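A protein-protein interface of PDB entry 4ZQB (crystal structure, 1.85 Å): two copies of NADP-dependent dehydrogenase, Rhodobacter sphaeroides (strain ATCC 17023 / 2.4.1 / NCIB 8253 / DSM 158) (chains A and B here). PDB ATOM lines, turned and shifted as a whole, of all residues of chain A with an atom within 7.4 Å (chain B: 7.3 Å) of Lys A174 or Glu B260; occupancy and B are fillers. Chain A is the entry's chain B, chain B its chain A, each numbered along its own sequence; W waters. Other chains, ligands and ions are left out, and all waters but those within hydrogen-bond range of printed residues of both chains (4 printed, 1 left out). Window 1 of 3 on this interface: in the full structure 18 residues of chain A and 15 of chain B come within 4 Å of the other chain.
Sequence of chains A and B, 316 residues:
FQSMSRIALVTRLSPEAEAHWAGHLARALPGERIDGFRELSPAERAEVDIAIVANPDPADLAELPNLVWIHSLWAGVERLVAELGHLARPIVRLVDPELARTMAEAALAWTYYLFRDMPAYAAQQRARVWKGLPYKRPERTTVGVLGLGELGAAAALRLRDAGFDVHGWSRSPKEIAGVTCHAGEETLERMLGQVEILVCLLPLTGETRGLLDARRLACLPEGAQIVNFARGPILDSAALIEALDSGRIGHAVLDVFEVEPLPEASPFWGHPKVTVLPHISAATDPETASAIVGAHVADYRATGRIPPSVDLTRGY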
ATOM      1  N   GLY A 147      14.161  28.389  21.990  1.00  0.00           N
ATOM      2  CA  GLY A 147      13.388  28.524  20.755  1.00  0.00           C
ATOM      3  C   GLY A 147      14.096  27.828  19.612  1.00  0.00           C
ATOM      4  O   GLY A 147      15.242  28.138  19.337  1.00  0.00           O
ATOM      5  N   LEU A 148      13.430  26.863  18.993  1.00  0.00           N
ATOM      6  CA  LEU A 148      13.954  26.179  17.815  1.00  0.00           C
ATOM      7  C   LEU A 148      13.019  26.306  16.620  1.00  0.00           C
ATOM      8  O   LEU A 148      12.752  25.316  15.946  1.00  0.00           O
ATOM      9  CB  LEU A 148      14.243  24.707  18.128  1.00  0.00           C
ATOM     10  CG  LEU A 148      15.267  24.511  19.244  1.00  0.00           C
ATOM     11  CD1 LEU A 148      15.305  23.058  19.653  1.00  0.00           C
ATOM     12  CD2 LEU A 148      16.648  24.974  18.770  1.00  0.00           C
ATOM     13  N   GLY A 149      12.590  27.531  16.354  1.00  0.00           N
ATOM     14  CA  GLY A 149      11.594  27.789  15.339  1.00  0.00           C
ATOM     15  C   GLY A 149      12.281  28.199  14.074  1.00  0.00           C
ATOM     16  O   GLY A 149      13.399  27.769  13.773  1.00  0.00           O
ATOM     17  N   ALA A 153      16.023  27.445  15.128  1.00  0.00           N
ATOM     18  CA  ALA A 153      16.671  26.271  14.550  1.00  0.00           C
ATOM     19  C   ALA A 153      17.795  26.647  13.571  1.00  0.00           C
ATOM     20  O   ALA A 153      18.852  25.982  13.496  1.00  0.00           O
ATOM     21  CB  ALA A 153      15.649  25.391  13.868  1.00  0.00           C
ATOM     22  N   GLY A 168      19.501  22.847  22.346  1.00  0.00           N
ATOM     23  CA  GLY A 168      18.364  23.668  22.011  1.00  0.00           C
ATOM     24  C   GLY A 168      17.198  23.276  22.884  1.00  0.00           C
ATOM     25  O   GLY A 168      17.148  22.132  23.395  1.00  0.00           O
ATOM     26  N   TRP A 169      16.278  24.222  23.083  1.00  0.00           N
ATOM     27  CA  TRP A 169      15.119  23.991  23.921  1.00  0.00           C
ATOM     28  C   TRP A 169      13.865  24.533  23.219  1.00  0.00           C
ATOM     29  O   TRP A 169      13.867  25.662  22.726  1.00  0.00           O
ATOM     30  CB  TRP A 169      15.280  24.695  25.283  1.00  0.00           C
ATOM     31  CG  TRP A 169      14.163  24.458  26.242  1.00  0.00           C
ATOM     32  CD1 TRP A 169      13.892  23.300  26.909  1.00  0.00           C
ATOM     33  CD2 TRP A 169      13.157  25.392  26.638  1.00  0.00           C
ATOM     34  NE1 TRP A 169      12.786  23.461  27.701  1.00  0.00           N
ATOM     35  CE2 TRP A 169      12.320  24.736  27.564  1.00  0.00           C
ATOM     36  CE3 TRP A 169      12.909  26.736  26.343  1.00  0.00           C
ATOM     37  CZ2 TRP A 169      11.245  25.377  28.183  1.00  0.00           C
ATOM     38  CZ3 TRP A 169      11.852  27.355  26.933  1.00  0.00           C
ATOM     39  CH2 TRP A 169      11.030  26.683  27.863  1.00  0.00           C
ATOM     40  N   SER A 170      12.810  23.733  23.197  1.00  0.00           N
ATOM     41  CA  SER A 170      11.541  24.153  22.628  1.00  0.00           C
ATOM     42  C   SER A 170      10.391  23.470  23.357  1.00  0.00           C
ATOM     43  O   SER A 170      10.606  22.705  24.278  1.00  0.00           O
ATOM     44  CB  SER A 170      11.486  23.859  21.114  1.00  0.00           C
ATOM     45  OG  SER A 170      11.379  22.448  20.879  1.00  0.00           O
ATOM     46  N   ARG A 171       9.158  23.782  22.968  1.00  0.00           N
ATOM     47  CA  ARG A 171       7.986  23.321  23.686  1.00  0.00           C
ATOM     48  C   ARG A 171       7.711  21.865  23.364  1.00  0.00           C
ATOM     49  O   ARG A 171       7.449  21.071  24.253  1.00  0.00           O
ATOM     50  CB  ARG A 171       6.775  24.189  23.282  1.00  0.00           C
ATOM     51  CG  ARG A 171       5.647  24.180  24.285  1.00  0.00           C
ATOM     52  CD  ARG A 171       4.661  25.309  23.977  1.00  0.00           C
ATOM     53  NE  ARG A 171       4.040  25.011  22.693  1.00  0.00           N
ATOM     54  CZ  ARG A 171       2.855  24.399  22.517  1.00  0.00           C
ATOM     55  NH1 ARG A 171       2.075  24.063  23.541  1.00  0.00           N
ATOM     56  NH2 ARG A 171       2.430  24.141  21.277  1.00  0.00           N
ATOM     57  N   SER A 172       7.833  21.510  22.090  1.00  0.00           N
ATOM     58  CA  SER A 172       7.618  20.162  21.634  1.00  0.00           C
ATOM     59  C   SER A 172       8.924  19.608  21.045  1.00  0.00           C
ATOM     60  O   SER A 172       9.811  20.359  20.645  1.00  0.00           O
ATOM     61  CB  SER A 172       6.545  20.151  20.568  1.00  0.00           C
ATOM     62  OG  SER A 172       7.012  20.880  19.439  1.00  0.00           O
ATOM     63  N   PRO A 173       9.039  18.287  20.999  1.00  0.00           N
ATOM     64  CA  PRO A 173      10.351  17.718  20.651  1.00  0.00           C
ATOM     65  C   PRO A 173      10.746  17.985  19.193  1.00  0.00           C
ATOM     66  O   PRO A 173       9.892  17.963  18.321  1.00  0.00           O
ATOM     67  CB  PRO A 173      10.191  16.204  20.917  1.00  0.00           C
ATOM     68  CG  PRO A 173       8.837  15.985  21.480  1.00  0.00           C
ATOM     69  CD  PRO A 173       8.037  17.254  21.325  1.00  0.00           C
ATOM     70  N   LYS A 174      12.038  18.226  18.991  1.00  0.00           N
ATOM     71  CA  LYS A 174      12.674  18.407  17.698  1.00  0.00           C
ATOM     72  C   LYS A 174      13.800  17.392  17.484  1.00  0.00           C
ATOM     73  O   LYS A 174      14.320  16.834  18.447  1.00  0.00           O
ATOM     74  CB  LYS A 174      13.369  19.747  17.648  1.00  0.00           C
ATOM     75  CG  LYS A 174      12.469  20.907  17.884  1.00  0.00           C
ATOM     76  CD  LYS A 174      11.766  21.323  16.597  1.00  0.00           C
ATOM     77  CE  LYS A 174      10.849  22.503  16.886  1.00  0.00           C
ATOM     78  NZ  LYS A 174       9.797  22.141  17.882  1.00  0.00           N
ATOM     79  N   GLU A 175      14.171  17.180  16.217  1.00  0.00           N
ATOM     80  CA  GLU A 175      15.406  16.484  15.850  1.00  0.00           C
ATOM     81  C   GLU A 175      16.162  17.408  14.929  1.00  0.00           C
ATOM     82  O   GLU A 175      15.676  17.745  13.830  1.00  0.00           O
ATOM     83  CB  GLU A 175      15.122  15.151  15.138  1.00  0.00           C
ATOM     84  CG  GLU A 175      14.376  14.195  16.037  1.00  0.00           C
ATOM     85  CD  GLU A 175      14.023  12.868  15.385  1.00  0.00           C
ATOM     86  OE1 GLU A 175      14.918  12.065  15.097  1.00  0.00           O
ATOM     87  OE2 GLU A 175      12.826  12.594  15.178  1.00  0.00           O
ATOM     88  N   ILE A 176      17.332  17.829  15.380  1.00  0.00           N
ATOM     89  CA  ILE A 176      18.214  18.704  14.631  1.00  0.00           C
ATOM     90  C   ILE A 176      19.610  18.047  14.557  1.00  0.00           C
ATOM     91  O   ILE A 176      20.248  17.713  15.602  1.00  0.00           O
ATOM     92  CB  ILE A 176      18.308  20.100  15.246  1.00  0.00           C
ATOM     93  CG1 ILE A 176      16.916  20.746  15.324  1.00  0.00           C
ATOM     94  CG2 ILE A 176      19.310  20.971  14.504  1.00  0.00           C
ATOM     95  CD1 ILE A 176      16.852  22.134  15.931  1.00  0.00           C
ATOM     96  N   ALA A 177      20.062  17.785  13.339  1.00  0.00           N
ATOM     97  CA  ALA A 177      21.343  17.088  13.172  1.00  0.00           C
ATOM     98  C   ALA A 177      22.465  17.808  13.912  1.00  0.00           C
ATOM     99  O   ALA A 177      22.613  19.021  13.791  1.00  0.00           O
ATOM    100  CB  ALA A 177      21.704  16.957  11.714  1.00  0.00           C
ATOM    101  N   VAL A 179      22.786  18.612  17.030  1.00  0.00           N
ATOM    102  CA  VAL A 179      22.338  19.485  18.141  1.00  0.00           C
ATOM    103  C   VAL A 179      21.594  18.627  19.119  1.00  0.00           C
ATOM    104  O   VAL A 179      20.784  17.773  18.714  1.00  0.00           O
ATOM    105  CB  VAL A 179      21.399  20.608  17.668  1.00  0.00           C
ATOM    106  CG1 VAL A 179      20.844  21.450  18.819  1.00  0.00           C
ATOM    107  CG2 VAL A 179      22.116  21.488  16.686  1.00  0.00           C
ATOM    108  N   THR A 180      21.845  18.858  20.421  1.00  0.00           N
ATOM    109  CA  THR A 180      21.126  18.114  21.471  1.00  0.00           C
ATOM    110  C   THR A 180      19.847  18.911  21.783  1.00  0.00           C
ATOM    111  O   THR A 180      19.918  20.047  22.263  1.00  0.00           O
ATOM    112  CB  THR A 180      21.987  17.906  22.753  1.00  0.00           C
ATOM    113  OG1 THR A 180      23.217  17.229  22.391  1.00  0.00           O
ATOM    114  CG2 THR A 180      21.250  17.051  23.784  1.00  0.00           C
ATOM    115  N   CYS A 181      18.690  18.319  21.523  1.00  0.00           N
ATOM    116  CA  CYS A 181      17.423  19.017  21.656  1.00  0.00           C
ATOM    117  C   CYS A 181      16.736  18.573  22.939  1.00  0.00           C
ATOM    118  O   CYS A 181      16.721  17.390  23.245  1.00  0.00           O
ATOM    119  CB  CYS A 181      16.556  18.716  20.456  1.00  0.00           C
ATOM    120  SG  CYS A 181      17.257  19.438  18.935  1.00  0.00           S
ATOM    121  N   HIS A 182      16.168  19.524  23.666  1.00  0.00           N
ATOM    122  CA  HIS A 182      15.388  19.305  24.892  1.00  0.00           C
ATOM    123  C   HIS A 182      14.011  19.901  24.709  1.00  0.00           C
ATOM    124  O   HIS A 182      13.867  20.901  24.026  1.00  0.00           O
ATOM    125  CB  HIS A 182      16.071  20.033  26.051  1.00  0.00           C
ATOM    126  CG  HIS A 182      17.475  19.586  26.240  1.00  0.00           C
ATOM    127  ND1 HIS A 182      17.802  18.427  26.911  1.00  0.00           N
ATOM    128  CD2 HIS A 182      18.639  20.110  25.810  1.00  0.00           C
ATOM    129  CE1 HIS A 182      19.111  18.251  26.878  1.00  0.00           C
ATOM    130  NE2 HIS A 182      19.636  19.254  26.207  1.00  0.00           N
ATOM    131  N   ALA A 183      13.009  19.312  25.351  1.00  0.00           N
ATOM    132  CA  ALA A 183      11.637  19.833  25.256  1.00  0.00           C
ATOM    133  C   ALA A 183      10.930  19.875  26.603  1.00  0.00           C
ATOM    134  O   ALA A 183      11.137  18.998  27.458  1.00  0.00           O
ATOM    135  CB  ALA A 183      10.799  19.034  24.268  1.00  0.00           C
ATOM    136  N   TYR A 316       1.337  32.054  19.391  1.00  0.00           N
ATOM    137  CA  TYR A 316       2.433  32.363  18.491  1.00  0.00           C
ATOM    138  C   TYR A 316       2.303  31.489  17.273  1.00  0.00           C
ATOM    139  O   TYR A 316       2.916  31.768  16.251  1.00  0.00           O
ATOM    140  CB  TYR A 316       3.810  32.157  19.189  1.00  0.00           C
ATOM    141  CG  TYR A 316       4.130  30.710  19.505  1.00  0.00           C
ATOM    142  CD1 TYR A 316       3.663  30.113  20.663  1.00  0.00           C
ATOM    143  CD2 TYR A 316       4.881  29.913  18.616  1.00  0.00           C
ATOM    144  CE1 TYR A 316       3.956  28.777  20.981  1.00  0.00           C
ATOM    145  CE2 TYR A 316       5.155  28.575  18.918  1.00  0.00           C
ATOM    146  CZ  TYR A 316       4.684  28.007  20.095  1.00  0.00           C
ATOM    147  OH  TYR A 316       4.958  26.693  20.397  1.00  0.00           O
ATOM    148  OXT TYR A 316       1.530  30.512  17.291  1.00  0.00           O
ATOM    149  N   ARG B  12      10.521  10.661  23.635  1.00  0.00           N
ATOM    150  CA  ARG B  12       9.894  11.970  23.470  1.00  0.00           C
ATOM    151  C   ARG B  12       8.894  11.852  22.344  1.00  0.00           C
ATOM    152  O   ARG B  12       8.769  12.729  21.492  1.00  0.00           O
ATOM    153  CB  ARG B  12      10.943  13.042  23.239  1.00  0.00           C
ATOM    154  CG  ARG B  12      11.746  13.315  24.491  1.00  0.00           C
ATOM    155  CD  ARG B  12      12.734  14.415  24.267  1.00  0.00           C
ATOM    156  NE  ARG B  12      13.800  14.035  23.354  1.00  0.00           N
ATOM    157  CZ  ARG B  12      14.977  14.648  23.274  1.00  0.00           C
ATOM    158  NH1 ARG B  12      15.272  15.681  24.062  1.00  0.00           N
ATOM    159  NH2 ARG B  12      15.894  14.213  22.408  1.00  0.00           N
ATOM    160  N   ASN B  55      14.084   8.447  20.664  1.00  0.00           N
ATOM    161  CA  ASN B  55      14.470   9.845  20.790  1.00  0.00           C
ATOM    162  C   ASN B  55      14.491  10.281  22.269  1.00  0.00           C
ATOM    163  O   ASN B  55      13.749  11.162  22.680  1.00  0.00           O
ATOM    164  CB  ASN B  55      13.540  10.746  19.945  1.00  0.00           C
ATOM    165  CG  ASN B  55      13.989  12.194  19.937  1.00  0.00           C
ATOM    166  OD1 ASN B  55      15.192  12.481  20.069  1.00  0.00           O
ATOM    167  ND2 ASN B  55      13.040  13.125  19.794  1.00  0.00           N
ATOM    168  N   ALA B 230      17.138   8.200   3.862  1.00  0.00           N
ATOM    169  CA  ALA B 230      18.239   7.974   4.773  1.00  0.00           C
ATOM    170  C   ALA B 230      18.232   9.010   5.928  1.00  0.00           C
ATOM    171  O   ALA B 230      17.474   8.866   6.892  1.00  0.00           O
ATOM    172  CB  ALA B 230      19.507   8.003   3.982  1.00  0.00           C
ATOM    173  N   ARG B 231      19.002  10.082   5.780  1.00  0.00           N
ATOM    174  CA  ARG B 231      18.989  11.220   6.669  1.00  0.00           C
ATOM    175  C   ARG B 231      19.219  12.461   5.824  1.00  0.00           C
ATOM    176  O   ARG B 231      19.916  12.416   4.795  1.00  0.00           O
ATOM    177  CB  ARG B 231      20.095  11.097   7.728  1.00  0.00           C
ATOM    178  CG  ARG B 231      19.864  10.006   8.781  1.00  0.00           C
ATOM    179  CD  ARG B 231      18.704  10.427   9.658  1.00  0.00           C
ATOM    180  NE  ARG B 231      18.445   9.566  10.822  1.00  0.00           N
ATOM    181  CZ  ARG B 231      17.559   8.573  10.870  1.00  0.00           C
ATOM    182  NH1 ARG B 231      16.841   8.203   9.798  1.00  0.00           N
ATOM    183  NH2 ARG B 231      17.419   7.916  12.011  1.00  0.00           N
ATOM    184  N   GLY B 232      18.655  13.578   6.250  1.00  0.00           N
ATOM    185  CA  GLY B 232      18.757  14.847   5.487  1.00  0.00           C
ATOM    186  C   GLY B 232      20.183  15.316   5.139  1.00  0.00           C
ATOM    187  O   GLY B 232      20.470  15.621   3.970  1.00  0.00           O
ATOM    188  N   PRO B 233      21.090  15.350   6.138  1.00  0.00           N
ATOM    189  CA  PRO B 233      22.455  15.860   5.931  1.00  0.00           C
ATOM    190  C   PRO B 233      23.310  15.106   4.892  1.00  0.00           C
ATOM    191  O   PRO B 233      24.377  15.586   4.514  1.00  0.00           O
ATOM    192  CB  PRO B 233      23.064  15.801   7.339  1.00  0.00           C
ATOM    193  CG  PRO B 233      21.874  15.972   8.246  1.00  0.00           C
ATOM    194  CD  PRO B 233      20.763  15.229   7.573  1.00  0.00           C
ATOM    195  N   ASP B 255      12.039  12.339   2.523  1.00  0.00           N
ATOM    196  CA  ASP B 255      11.369  11.874   3.728  1.00  0.00           C
ATOM    197  C   ASP B 255      12.081  12.337   4.986  1.00  0.00           C
ATOM    198  O   ASP B 255      11.551  12.134   6.097  1.00  0.00           O
ATOM    199  CB  ASP B 255      11.357  10.325   3.666  1.00  0.00           C
ATOM    200  CG  ASP B 255      10.501   9.662   4.723  1.00  0.00           C
ATOM    201  OD1 ASP B 255       9.348  10.135   4.919  1.00  0.00           O
ATOM    202  OD2 ASP B 255      10.944   8.626   5.350  1.00  0.00           O
ATOM    203  N   VAL B 256      13.298  12.862   4.853  1.00  0.00           N
ATOM    204  CA  VAL B 256      14.201  13.093   5.996  1.00  0.00           C
ATOM    205  C   VAL B 256      14.957  14.416   5.771  1.00  0.00           C
ATOM    206  O   VAL B 256      15.231  14.794   4.605  1.00  0.00           O
ATOM    207  CB  VAL B 256      15.211  11.947   6.221  1.00  0.00           C
ATOM    208  CG1 VAL B 256      14.488  10.705   6.725  1.00  0.00           C
ATOM    209  CG2 VAL B 256      16.032  11.658   4.940  1.00  0.00           C
ATOM    210  N   PHE B 257      15.137  15.168   6.866  1.00  0.00           N
ATOM    211  CA  PHE B 257      15.639  16.538   6.796  1.00  0.00           C
ATOM    212  C   PHE B 257      16.531  16.858   7.988  1.00  0.00           C
ATOM    213  O   PHE B 257      16.465  16.198   9.017  1.00  0.00           O
ATOM    214  CB  PHE B 257      14.475  17.523   6.713  1.00  0.00           C
ATOM    215  CG  PHE B 257      13.497  17.201   5.627  1.00  0.00           C
ATOM    216  CD1 PHE B 257      12.418  16.343   5.877  1.00  0.00           C
ATOM    217  CD2 PHE B 257      13.644  17.723   4.370  1.00  0.00           C
ATOM    218  CE1 PHE B 257      11.527  16.013   4.883  1.00  0.00           C
ATOM    219  CE2 PHE B 257      12.733  17.409   3.346  1.00  0.00           C
ATOM    220  CZ  PHE B 257      11.674  16.562   3.611  1.00  0.00           C
ATOM    221  N   GLU B 258      17.374  17.877   7.838  1.00  0.00           N
ATOM    222  CA  GLU B 258      18.316  18.273   8.903  1.00  0.00           C
ATOM    223  C   GLU B 258      17.603  18.755  10.165  1.00  0.00           C
ATOM    224  O   GLU B 258      18.055  18.495  11.251  1.00  0.00           O
ATOM    225  CB  GLU B 258      19.268  19.301   8.308  1.00  0.00           C
ATOM    226  CG  GLU B 258      20.250  19.881   9.236  1.00  0.00           C
ATOM    227  CD  GLU B 258      21.348  20.619   8.491  1.00  0.00           C
ATOM    228  OE1 GLU B 258      20.983  21.483   7.626  1.00  0.00           O
ATOM    229  OE2 GLU B 258      22.536  20.309   8.790  1.00  0.00           O
ATOM    230  N   VAL B 259      16.445  19.385   9.988  1.00  0.00           N
ATOM    231  CA  VAL B 259      15.554  19.796  11.065  1.00  0.00           C
ATOM    232  C   VAL B 259      14.161  19.200  10.795  1.00  0.00           C
ATOM    233  O   VAL B 259      13.617  19.358   9.689  1.00  0.00           O
ATOM    234  CB  VAL B 259      15.445  21.326  11.121  1.00  0.00           C
ATOM    235  CG1 VAL B 259      14.507  21.750  12.244  1.00  0.00           C
ATOM    236  CG2 VAL B 259      16.825  21.958  11.279  1.00  0.00           C
ATOM    237  N   GLU B 260      13.645  18.457  11.765  1.00  0.00           N
ATOM    238  CA  GLU B 260      12.325  17.858  11.722  1.00  0.00           C
ATOM    239  C   GLU B 260      11.573  18.209  13.003  1.00  0.00           C
ATOM    240  O   GLU B 260      12.129  18.074  14.064  1.00  0.00           O
ATOM    241  CB  GLU B 260      12.398  16.335  11.560  1.00  0.00           C
ATOM    242  CG  GLU B 260      13.032  15.887  10.237  1.00  0.00           C
ATOM    243  CD  GLU B 260      13.213  14.373  10.100  1.00  0.00           C
ATOM    244  OE1 GLU B 260      12.636  13.609  10.890  1.00  0.00           O
ATOM    245  OE2 GLU B 260      13.985  13.921   9.218  1.00  0.00           O
ATOM    246  N   PRO B 261      10.331  18.675  12.936  1.00  0.00           N
ATOM    247  CA  PRO B 261       9.568  18.907  11.673  1.00  0.00           C
ATOM    248  C   PRO B 261      10.211  19.953  10.780  1.00  0.00           C
ATOM    249  O   PRO B 261      10.834  20.907  11.266  1.00  0.00           O
ATOM    250  CB  PRO B 261       8.212  19.406  12.163  1.00  0.00           C
ATOM    251  CG  PRO B 261       8.116  18.945  13.594  1.00  0.00           C
ATOM    252  CD  PRO B 261       9.523  18.932  14.133  1.00  0.00           C
ATOM    253  N   LEU B 262      10.089  19.746   9.481  1.00  0.00           N
ATOM    254  CA  LEU B 262      10.657  20.645   8.479  1.00  0.00           C
ATOM    255  C   LEU B 262      10.162  22.049   8.727  1.00  0.00           C
ATOM    256  O   LEU B 262       8.929  22.267   8.746  1.00  0.00           O
ATOM    257  CB  LEU B 262      10.272  20.201   7.062  1.00  0.00           C
ATOM    258  CG  LEU B 262      10.863  20.981   5.901  1.00  0.00           C
ATOM    259  CD1 LEU B 262      12.387  20.866   5.898  1.00  0.00           C
ATOM    260  CD2 LEU B 262      10.301  20.460   4.581  1.00  0.00           C
ATOM    261  N   PRO B 263      11.099  23.009   8.955  1.00  0.00           N
ATOM    262  CA  PRO B 263      10.621  24.391   9.148  1.00  0.00           C
ATOM    263  C   PRO B 263       9.775  24.910   7.984  1.00  0.00           C
ATOM    264  O   PRO B 263      10.034  24.607   6.822  1.00  0.00           O
ATOM    265  CB  PRO B 263      11.910  25.204   9.253  1.00  0.00           C
ATOM    266  CG  PRO B 263      12.908  24.233   9.780  1.00  0.00           C
ATOM    267  CD  PRO B 263      12.555  22.929   9.091  1.00  0.00           C
ATOM    268  N   LEU B 277       7.733  14.126   2.511  1.00  0.00           N
ATOM    269  CA  LEU B 277       7.099  13.102   3.322  1.00  0.00           C
ATOM    270  C   LEU B 277       7.605  13.292   4.723  1.00  0.00           C
ATOM    271  O   LEU B 277       8.800  13.587   4.905  1.00  0.00           O
ATOM    272  CB  LEU B 277       7.466  11.714   2.834  1.00  0.00           C
ATOM    273  CG  LEU B 277       7.072  11.398   1.403  1.00  0.00           C
ATOM    274  CD1 LEU B 277       7.671  10.042   1.020  1.00  0.00           C
ATOM    275  CD2 LEU B 277       5.539  11.406   1.164  1.00  0.00           C
ATOM    276  N   PRO B 278       6.747  13.112   5.735  1.00  0.00           N
ATOM    277  CA  PRO B 278       7.193  13.410   7.139  1.00  0.00           C
ATOM    278  C   PRO B 278       7.859  12.256   7.902  1.00  0.00           C
ATOM    279  O   PRO B 278       7.413  11.878   8.979  1.00  0.00           O
ATOM    280  CB  PRO B 278       5.900  13.834   7.805  1.00  0.00           C
ATOM    281  CG  PRO B 278       4.831  13.031   7.096  1.00  0.00           C
ATOM    282  CD  PRO B 278       5.294  12.920   5.677  1.00  0.00           C
ATOM    283  N   HIS B 279       8.946  11.742   7.350  1.00  0.00           N
ATOM    284  CA  HIS B 279       9.723  10.684   7.975  1.00  0.00           C
ATOM    285  C   HIS B 279       8.841   9.464   8.266  1.00  0.00           C
ATOM    286  O   HIS B 279       8.703   9.026   9.410  1.00  0.00           O
ATOM    287  CB  HIS B 279      10.399  11.205   9.231  1.00  0.00           C
ATOM    288  CG  HIS B 279      11.565  10.396   9.670  1.00  0.00           C
ATOM    289  ND1 HIS B 279      12.676  10.964  10.246  1.00  0.00           N
ATOM    290  CD2 HIS B 279      11.828   9.070   9.567  1.00  0.00           C
ATOM    291  CE1 HIS B 279      13.558  10.015  10.528  1.00  0.00           C
ATOM    292  NE2 HIS B 279      13.070   8.858  10.116  1.00  0.00           N
HETATM  293  O   HOH W   1      10.770  15.909  15.803  1.00  0.00           O
HETATM  294  O   HOH W   2      13.676  16.677  26.517  1.00  0.00           O
HETATM  295  O   HOH W   3      15.454  13.917  12.191  1.00  0.00           O
HETATM  296  O   HOH W   4      11.082  13.186  12.976  1.00  0.00           O
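NH2 of Arg B12 sits close to O of Cys A181 (3.4 Å). The backbone carbonyl oxygen (O) of Glu B258 sits at hydrogen-bond distance from the backbone NH (N) of Ala A177 (3.0 Å). The backbone NH (N) of Glu B260 lies within hydrogen-bond range of the backbone carbonyl oxygen (O) of Glu A175 (3.0 Å).
The guanidinium group of Arg B12 lies within hydrogen-bond range of the backbone carbonyl oxygen of Asn B55, 3.0 Å away. ND1 of His B279 lies within hydrogen-bond range of OE1 of Glu B260, at 2.7 Å. O of Gly A168 sits at hydrogen-bond distance from N of His A182, 2.8 Å away. OG of Ser A170 is in hydrogen-bond range of NZ of Lys A174, 3.4 Å away. The backbone NH (N) of Ser A170 sits at hydrogen-bond distance from the backbone carbonyl oxygen (O) of His A182, at 3.1 Å. The backbone carbonyl oxygen (O) of Ser A172 is in hydrogen-bond range of the side-chain amino group (NZ) of Lys A174 (3.3 Å).
Pro A173 touches Arg B12. Glu B260 touches Lys A174. Glu A175 touches Glu B258. O of Glu A175 touches CA of Val B259, at 3.4 Å. CA of Ile A176 touches O of Glu B258 (3.4 Å). CG of Pro B233 touches CB of Ala A177, at 3.6 Å. Arg B12 touches His A182.
Gly A168 touches none of the printed residues of chain B. Printed residues of chain B within 4 Å of Pro A173: Arg B12 (3.3 Å). Of chain B, only Glu B260 comes within 4 Å of Lys A174. Printed residues of chain B within 4 Å of Ala A177: Pro B233 (3.6 Å) and Glu B258 (3.0 Å). Of the printed residues of chain B, His A182 touches Arg B12 (3.7 Å). Glu B260 touches just these residues of chain A: Lys A174 and Glu A175. The nearest residue of chain B that does not touch Lys A174 is Pro B261 (4.1 Å). The nearest residue of chain A that does not touch Glu B260 is Pro A173 (4.8 Å). The nearest printed residue of chain B that does not touch Glu A175 is Asn B55 (4.1 Å).
Of the 18 printed residues of chain B, 5 touch a printed residue of chain A. Hydrophobic or aromatic side chains of chain B within 4 Å of the printed part of chain A: Pro B233. Printed residues of chain A that touch a printed residue of chain B: Pro A173, Lys A174, Glu A175, Ile A176, Ala A177, Cys A181 and His A182. Among the printed residues, no Asp or Glu carboxylate lies within 4 Å of a Lys or Arg side-chain nitrogen of the other chain.
No position is printed for both chains.
Water W4 lies within hydrogen-bond range of the side-chain carboxylate (OE1) of Glu B260 and the side-chain carboxylate (OE2) of Glu A175. Water W2 lies within hydrogen-bond range of the backbone NH of Ala A183 (3.0 Å) and the guanidinium group of Arg B12 (3.1 Å). Water W1 bridges O of Glu B260 (3.1 Å) and O of Pro A173 (3.4 Å). Water W3 bridges OE1 of Glu B260 (3.1 Å) and OE1 of Glu A175 (3.5 Å).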
